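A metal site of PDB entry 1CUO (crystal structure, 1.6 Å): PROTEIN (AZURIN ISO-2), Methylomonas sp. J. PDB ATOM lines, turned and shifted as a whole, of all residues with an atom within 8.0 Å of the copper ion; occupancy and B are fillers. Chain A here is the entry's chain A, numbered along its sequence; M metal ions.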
ATOM      1  N   SER A   9     -33.957  24.578  -0.688  1.00  0.00           N
ATOM      2  CA  SER A   9     -33.216  23.456  -0.152  1.00  0.00           C
ATOM      3  C   SER A   9     -33.679  23.274   1.297  1.00  0.00           C
ATOM      4  O   SER A   9     -34.452  24.067   1.812  1.00  0.00           O
ATOM      5  CB  SER A   9     -31.709  23.669  -0.192  1.00  0.00           C
ATOM      6  OG  SER A   9     -31.331  24.788   0.651  1.00  0.00           O
ATOM      7  N   GLY A  10     -33.233  22.200   1.936  1.00  0.00           N
ATOM      8  CA  GLY A  10     -33.686  22.009   3.334  1.00  0.00           C
ATOM      9  C   GLY A  10     -32.661  21.114   3.970  1.00  0.00           C
ATOM     10  O   GLY A  10     -31.461  21.144   3.679  1.00  0.00           O
ATOM     11  N   THR A  12     -31.986  18.072   3.564  1.00  0.00           N
ATOM     12  CA  THR A  12     -31.617  16.976   2.695  1.00  0.00           C
ATOM     13  C   THR A  12     -30.561  17.431   1.698  1.00  0.00           C
ATOM     14  O   THR A  12     -30.116  18.593   1.742  1.00  0.00           O
ATOM     15  CB  THR A  12     -32.832  16.516   1.870  1.00  0.00           C
ATOM     16  OG1 THR A  12     -33.180  17.564   0.941  1.00  0.00           O
ATOM     17  CG2 THR A  12     -34.069  16.274   2.729  1.00  0.00           C
ATOM     18  N   MET A  13     -30.124  16.545   0.805  1.00  0.00           N
ATOM     19  CA  MET A  13     -29.140  16.974  -0.201  1.00  0.00           C
ATOM     20  C   MET A  13     -29.750  17.063  -1.591  1.00  0.00           C
ATOM     21  O   MET A  13     -29.164  16.600  -2.566  1.00  0.00           O
ATOM     22  CB  MET A  13     -27.896  16.085  -0.182  1.00  0.00           C
ATOM     23  CG  MET A  13     -27.012  16.329   1.041  1.00  0.00           C
ATOM     24  SD  MET A  13     -25.537  15.307   1.015  1.00  0.00           S
ATOM     25  CE  MET A  13     -25.253  15.150   2.779  1.00  0.00           C
ATOM     26  N   THR A  14     -30.893  17.702  -1.717  1.00  0.00           N
ATOM     27  CA  THR A  14     -31.628  17.924  -2.940  1.00  0.00           C
ATOM     28  C   THR A  14     -32.088  19.380  -3.099  1.00  0.00           C
ATOM     29  O   THR A  14     -32.530  19.997  -2.133  1.00  0.00           O
ATOM     30  CB  THR A  14     -32.938  17.096  -2.944  1.00  0.00           C
ATOM     31  OG1 THR A  14     -33.775  17.522  -1.846  1.00  0.00           O
ATOM     32  CG2 THR A  14     -32.718  15.604  -2.864  1.00  0.00           C
ATOM     33  N   TYR A  15     -32.088  19.915  -4.308  1.00  0.00           N
ATOM     34  CA  TYR A  15     -32.688  21.193  -4.621  1.00  0.00           C
ATOM     35  C   TYR A  15     -34.150  20.949  -4.985  1.00  0.00           C
ATOM     36  O   TYR A  15     -34.531  19.858  -5.423  1.00  0.00           O
ATOM     37  CB  TYR A  15     -32.018  21.869  -5.823  1.00  0.00           C
ATOM     38  CG  TYR A  15     -30.606  22.386  -5.635  1.00  0.00           C
ATOM     39  CD1 TYR A  15     -30.382  23.466  -4.773  1.00  0.00           C
ATOM     40  CD2 TYR A  15     -29.540  21.897  -6.364  1.00  0.00           C
ATOM     41  CE1 TYR A  15     -29.103  24.002  -4.624  1.00  0.00           C
ATOM     42  CE2 TYR A  15     -28.251  22.401  -6.222  1.00  0.00           C
ATOM     43  CZ  TYR A  15     -28.066  23.474  -5.371  1.00  0.00           C
ATOM     44  OH  TYR A  15     -26.794  23.995  -5.262  1.00  0.00           O
ATOM     45  N   PHE A  33     -32.289  31.949  -3.261  1.00  0.00           N
ATOM     46  CA  PHE A  33     -32.016  30.592  -2.765  1.00  0.00           C
ATOM     47  C   PHE A  33     -32.348  30.589  -1.291  1.00  0.00           C
ATOM     48  O   PHE A  33     -31.916  31.475  -0.583  1.00  0.00           O
ATOM     49  CB  PHE A  33     -30.563  30.248  -3.044  1.00  0.00           C
ATOM     50  CG  PHE A  33     -30.134  28.898  -2.531  1.00  0.00           C
ATOM     51  CD1 PHE A  33     -29.100  28.781  -1.631  1.00  0.00           C
ATOM     52  CD2 PHE A  33     -30.832  27.745  -2.920  1.00  0.00           C
ATOM     53  CE1 PHE A  33     -28.712  27.537  -1.148  1.00  0.00           C
ATOM     54  CE2 PHE A  33     -30.443  26.528  -2.424  1.00  0.00           C
ATOM     55  CZ  PHE A  33     -29.400  26.393  -1.535  1.00  0.00           C
ATOM     56  N   HIS A  35     -33.113  28.257   2.445  1.00  0.00           N
ATOM     57  CA  HIS A  35     -32.883  26.964   3.147  1.00  0.00           C
ATOM     58  C   HIS A  35     -33.997  26.839   4.183  1.00  0.00           C
ATOM     59  O   HIS A  35     -34.063  27.645   5.101  1.00  0.00           O
ATOM     60  CB  HIS A  35     -31.510  27.004   3.802  1.00  0.00           C
ATOM     61  CG  HIS A  35     -31.062  25.736   4.443  1.00  0.00           C
ATOM     62  ND1 HIS A  35     -31.917  24.908   5.152  1.00  0.00           N
ATOM     63  CD2 HIS A  35     -29.811  25.216   4.557  1.00  0.00           C
ATOM     64  CE1 HIS A  35     -31.186  23.919   5.665  1.00  0.00           C
ATOM     65  NE2 HIS A  35     -29.907  24.063   5.308  1.00  0.00           N
ATOM     66  N   GLY A  43     -22.806  21.848   9.413  1.00  0.00           N
ATOM     67  CA  GLY A  43     -23.330  20.519   9.248  1.00  0.00           C
ATOM     68  C   GLY A  43     -24.338  20.406   8.119  1.00  0.00           C
ATOM     69  O   GLY A  43     -24.428  19.343   7.514  1.00  0.00           O
ATOM     70  N   MET A  44     -25.092  21.474   7.832  1.00  0.00           N
ATOM     71  CA  MET A  44     -26.108  21.326   6.782  1.00  0.00           C
ATOM     72  C   MET A  44     -26.182  22.599   5.923  1.00  0.00           C
ATOM     73  O   MET A  44     -27.258  23.048   5.564  1.00  0.00           O
ATOM     74  CB  MET A  44     -27.458  20.965   7.362  1.00  0.00           C
ATOM     75  CG  MET A  44     -28.503  20.533   6.343  1.00  0.00           C
ATOM     76  SD  MET A  44     -27.903  19.254   5.229  1.00  0.00           S
ATOM     77  CE  MET A  44     -27.459  17.988   6.420  1.00  0.00           C
ATOM     78  N   GLY A  45     -25.022  23.170   5.675  1.00  0.00           N
ATOM     79  CA  GLY A  45     -25.011  24.391   4.861  1.00  0.00           C
ATOM     80  C   GLY A  45     -25.209  24.024   3.386  1.00  0.00           C
ATOM     81  O   GLY A  45     -24.769  22.973   2.921  1.00  0.00           O
ATOM     82  N   HIS A  46     -25.758  24.976   2.636  1.00  0.00           N
ATOM     83  CA  HIS A  46     -25.900  24.783   1.195  1.00  0.00           C
ATOM     84  C   HIS A  46     -25.617  26.120   0.508  1.00  0.00           C
ATOM     85  O   HIS A  46     -25.886  27.198   1.046  1.00  0.00           O
ATOM     86  CB  HIS A  46     -27.313  24.410   0.720  1.00  0.00           C
ATOM     87  CG  HIS A  46     -27.892  23.151   1.328  1.00  0.00           C
ATOM     88  ND1 HIS A  46     -27.294  21.949   1.172  1.00  0.00           N
ATOM     89  CD2 HIS A  46     -29.020  22.965   2.053  1.00  0.00           C
ATOM     90  CE1 HIS A  46     -28.043  21.018   1.764  1.00  0.00           C
ATOM     91  NE2 HIS A  46     -29.097  21.620   2.308  1.00  0.00           N
ATOM     92  N   ASN A  47     -25.155  25.975  -0.752  1.00  0.00           N
ATOM     93  CA  ASN A  47     -25.007  27.177  -1.578  1.00  0.00           C
ATOM     94  C   ASN A  47     -25.439  26.787  -3.004  1.00  0.00           C
ATOM     95  O   ASN A  47     -25.913  25.658  -3.166  1.00  0.00           O
ATOM     96  CB  ASN A  47     -23.620  27.805  -1.613  1.00  0.00           C
ATOM     97  CG  ASN A  47     -22.545  26.844  -2.054  1.00  0.00           C
ATOM     98  OD1 ASN A  47     -22.797  25.708  -2.487  1.00  0.00           O
ATOM     99  ND2 ASN A  47     -21.241  27.195  -1.994  1.00  0.00           N
ATOM    100  N   TRP A  48     -25.318  27.728  -3.931  1.00  0.00           N
ATOM    101  CA  TRP A  48     -25.746  27.504  -5.329  1.00  0.00           C
ATOM    102  C   TRP A  48     -24.574  28.082  -6.147  1.00  0.00           C
ATOM    103  O   TRP A  48     -24.268  29.269  -5.960  1.00  0.00           O
ATOM    104  CB  TRP A  48     -27.036  28.234  -5.588  1.00  0.00           C
ATOM    105  CG  TRP A  48     -27.605  28.013  -6.977  1.00  0.00           C
ATOM    106  CD1 TRP A  48     -28.541  27.084  -7.316  1.00  0.00           C
ATOM    107  CD2 TRP A  48     -27.322  28.798  -8.132  1.00  0.00           C
ATOM    108  NE1 TRP A  48     -28.860  27.236  -8.655  1.00  0.00           N
ATOM    109  CE2 TRP A  48     -28.079  28.243  -9.185  1.00  0.00           C
ATOM    110  CE3 TRP A  48     -26.483  29.877  -8.418  1.00  0.00           C
ATOM    111  CZ2 TRP A  48     -28.054  28.734 -10.490  1.00  0.00           C
ATOM    112  CZ3 TRP A  48     -26.457  30.368  -9.723  1.00  0.00           C
ATOM    113  CH2 TRP A  48     -27.224  29.811 -10.733  1.00  0.00           C
ATOM    114  N   ILE A  86     -22.774  30.242   1.431  1.00  0.00           N
ATOM    115  CA  ILE A  86     -23.404  29.150   2.175  1.00  0.00           C
ATOM    116  C   ILE A  86     -24.437  29.729   3.143  1.00  0.00           C
ATOM    117  O   ILE A  86     -24.256  30.713   3.910  1.00  0.00           O
ATOM    118  CB  ILE A  86     -22.301  28.404   2.964  1.00  0.00           C
ATOM    119  CG1 ILE A  86     -21.337  27.713   2.018  1.00  0.00           C
ATOM    120  CG2 ILE A  86     -22.900  27.412   3.955  1.00  0.00           C
ATOM    121  CD1 ILE A  86     -21.836  26.399   1.395  1.00  0.00           C
ATOM    122  N   ILE A  87     -25.586  29.081   3.245  1.00  0.00           N
ATOM    123  CA  ILE A  87     -26.677  29.394   4.131  1.00  0.00           C
ATOM    124  C   ILE A  87     -27.118  28.122   4.861  1.00  0.00           C
ATOM    125  O   ILE A  87     -26.929  27.044   4.369  1.00  0.00           O
ATOM    126  CB  ILE A  87     -27.915  30.055   3.491  1.00  0.00           C
ATOM    127  CG1 ILE A  87     -28.433  29.234   2.307  1.00  0.00           C
ATOM    128  CG2 ILE A  87     -27.559  31.474   2.984  1.00  0.00           C
ATOM    129  CD1 ILE A  87     -29.695  29.800   1.680  1.00  0.00           C
ATOM    130  N   PHE A 111     -24.641  23.625  -8.668  1.00  0.00           N
ATOM    131  CA  PHE A 111     -24.424  22.570  -7.697  1.00  0.00           C
ATOM    132  C   PHE A 111     -24.023  23.211  -6.362  1.00  0.00           C
ATOM    133  O   PHE A 111     -23.799  24.413  -6.329  1.00  0.00           O
ATOM    134  CB  PHE A 111     -23.278  21.631  -8.114  1.00  0.00           C
ATOM    135  CG  PHE A 111     -21.947  22.367  -8.281  1.00  0.00           C
ATOM    136  CD1 PHE A 111     -21.730  23.092  -9.460  1.00  0.00           C
ATOM    137  CD2 PHE A 111     -20.984  22.336  -7.302  1.00  0.00           C
ATOM    138  CE1 PHE A 111     -20.545  23.787  -9.637  1.00  0.00           C
ATOM    139  CE2 PHE A 111     -19.778  23.012  -7.496  1.00  0.00           C
ATOM    140  CZ  PHE A 111     -19.592  23.743  -8.646  1.00  0.00           C
ATOM    141  N   CYS A 112     -24.104  22.390  -5.335  1.00  0.00           N
ATOM    142  CA  CYS A 112     -23.717  22.859  -3.973  1.00  0.00           C
ATOM    143  C   CYS A 112     -22.306  22.436  -3.685  1.00  0.00           C
ATOM    144  O   CYS A 112     -21.948  21.260  -3.870  1.00  0.00           O
ATOM    145  CB  CYS A 112     -24.729  22.190  -3.028  1.00  0.00           C
ATOM    146  SG  CYS A 112     -24.414  22.595  -1.271  1.00  0.00           S
ATOM    147  N   SER A 113     -21.391  23.334  -3.187  1.00  0.00           N
ATOM    148  CA  SER A 113     -20.032  22.959  -2.985  1.00  0.00           C
ATOM    149  C   SER A 113     -19.654  22.633  -1.514  1.00  0.00           C
ATOM    150  O   SER A 113     -18.470  22.400  -1.327  1.00  0.00           O
ATOM    151  CB  SER A 113     -19.010  24.001  -3.509  1.00  0.00           C
ATOM    152  OG  SER A 113     -19.264  25.237  -2.907  1.00  0.00           O
ATOM    153  N   TYR A 114     -20.664  22.623  -0.658  1.00  0.00           N
ATOM    154  CA  TYR A 114     -20.360  22.196   0.737  1.00  0.00           C
ATOM    155  C   TYR A 114     -19.813  20.785   0.620  1.00  0.00           C
ATOM    156  O   TYR A 114     -20.409  19.953  -0.100  1.00  0.00           O
ATOM    157  CB  TYR A 114     -21.703  22.206   1.485  1.00  0.00           C
ATOM    158  CG  TYR A 114     -21.552  21.871   2.957  1.00  0.00           C
ATOM    159  CD1 TYR A 114     -21.571  20.528   3.360  1.00  0.00           C
ATOM    160  CD2 TYR A 114     -21.405  22.864   3.897  1.00  0.00           C
ATOM    161  CE1 TYR A 114     -21.436  20.214   4.698  1.00  0.00           C
ATOM    162  CE2 TYR A 114     -21.246  22.542   5.249  1.00  0.00           C
ATOM    163  CZ  TYR A 114     -21.282  21.216   5.619  1.00  0.00           C
ATOM    164  OH  TYR A 114     -21.135  20.899   6.964  1.00  0.00           O
ATOM    165  N   PRO A 115     -18.751  20.448   1.321  1.00  0.00           N
ATOM    166  CA  PRO A 115     -18.134  19.140   1.244  1.00  0.00           C
ATOM    167  C   PRO A 115     -19.137  18.000   1.284  1.00  0.00           C
ATOM    168  O   PRO A 115     -20.025  17.915   2.123  1.00  0.00           O
ATOM    169  CB  PRO A 115     -17.202  19.109   2.462  1.00  0.00           C
ATOM    170  CG  PRO A 115     -16.776  20.532   2.597  1.00  0.00           C
ATOM    171  CD  PRO A 115     -17.970  21.362   2.206  1.00  0.00           C
ATOM    172  N   GLY A 116     -19.064  17.183   0.219  1.00  0.00           N
ATOM    173  CA  GLY A 116     -19.898  16.008   0.101  1.00  0.00           C
ATOM    174  C   GLY A 116     -21.274  16.178  -0.487  1.00  0.00           C
ATOM    175  O   GLY A 116     -22.008  15.172  -0.534  1.00  0.00           O
ATOM    176  N   HIS A 117     -21.713  17.360  -0.892  1.00  0.00           N
ATOM    177  CA  HIS A 117     -23.042  17.582  -1.430  1.00  0.00           C
ATOM    178  C   HIS A 117     -23.115  17.580  -2.948  1.00  0.00           C
ATOM    179  O   HIS A 117     -24.189  17.353  -3.519  1.00  0.00           O
ATOM    180  CB  HIS A 117     -23.545  18.961  -0.947  1.00  0.00           C
ATOM    181  CG  HIS A 117     -23.913  19.023   0.510  1.00  0.00           C
ATOM    182  ND1 HIS A 117     -24.733  20.012   0.999  1.00  0.00           N
ATOM    183  CD2 HIS A 117     -23.593  18.247   1.569  1.00  0.00           C
ATOM    184  CE1 HIS A 117     -24.879  19.866   2.300  1.00  0.00           C
ATOM    185  NE2 HIS A 117     -24.207  18.786   2.689  1.00  0.00           N
ATOM    186  N   PHE A 118     -21.983  17.846  -3.634  1.00  0.00           N
ATOM    187  CA  PHE A 118     -22.092  18.022  -5.080  1.00  0.00           C
ATOM    188  C   PHE A 118     -22.607  16.829  -5.851  1.00  0.00           C
ATOM    189  O   PHE A 118     -23.332  17.089  -6.827  1.00  0.00           O
ATOM    190  CB  PHE A 118     -20.826  18.602  -5.697  1.00  0.00           C
ATOM    191  CG  PHE A 118     -19.834  17.675  -6.323  1.00  0.00           C
ATOM    192  CD1 PHE A 118     -19.001  16.872  -5.576  1.00  0.00           C
ATOM    193  CD2 PHE A 118     -19.741  17.616  -7.708  1.00  0.00           C
ATOM    194  CE1 PHE A 118     -18.089  16.022  -6.196  1.00  0.00           C
ATOM    195  CE2 PHE A 118     -18.828  16.795  -8.329  1.00  0.00           C
ATOM    196  CZ  PHE A 118     -18.012  15.987  -7.569  1.00  0.00           C
ATOM    197  N   MET A 121     -26.643  17.052  -5.165  1.00  0.00           N
ATOM    198  CA  MET A 121     -27.202  18.396  -5.223  1.00  0.00           C
ATOM    199  C   MET A 121     -26.646  19.143  -6.422  1.00  0.00           C
ATOM    200  O   MET A 121     -25.653  19.868  -6.378  1.00  0.00           O
ATOM    201  CB  MET A 121     -26.867  19.042  -3.876  1.00  0.00           C
ATOM    202  CG  MET A 121     -27.740  20.231  -3.557  1.00  0.00           C
ATOM    203  SD  MET A 121     -27.750  20.409  -1.729  1.00  0.00           S
ATOM    204  CE  MET A 121     -28.978  21.709  -1.687  1.00  0.00           C
HETATM  205 CU    CU M   1     -25.623  21.569   0.013  1.00  0.00          CU
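The copper ion is bound by the side-chain sulfur of Cys 112 (2.0 Å), a ring nitrogen (ND1) of His 117 (2.0 Å) and a ring nitrogen (ND1) of His 46 (2.1 Å). The copper ion has three donor atoms within binding distance. Slightly farther from the copper ion lies the side-chain sulfur (SD) of Met 121 (3.0 Å).
Gly 45 touches the copper ion. Five residues have an atom within 4 Å of the copper ion: Gly 45, His 46, Cys 112, His 117 and Met 121. The nearest printed residue that does not touch the copper ion is Tyr 114 (4.2 Å).
The backbone NH (N) of Cys 112 lies within hydrogen-bond range of the backbone carbonyl oxygen (O) of Met 121, 3.1 Å away. The side-chain sulfur (SG) of Cys 112 sits close to the backbone NH (N) of Tyr 114 (3.8 Å). The backbone NH (N) of Asn 47 sits close to the side-chain sulfur (SG) of Cys 112 (3.5 Å). The backbone NH of Cys 112 lies within hydrogen-bond range of the side-chain hydroxyl of Tyr 15 (3.1 Å). A ring nitrogen (ND1) of His 46 sits close to the side-chain sulfur (SD) of Met 121, 3.3 Å away. A ring nitrogen (NE2) of His 46 lies close to the backbone carbonyl oxygen of Thr 12 (3.2 Å). NE2 of His 46 sits at hydrogen-bond distance from O of Gly 10, at 2.8 Å. N of Ile 87 sits at hydrogen-bond distance from O of His 46, at 2.9 Å.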
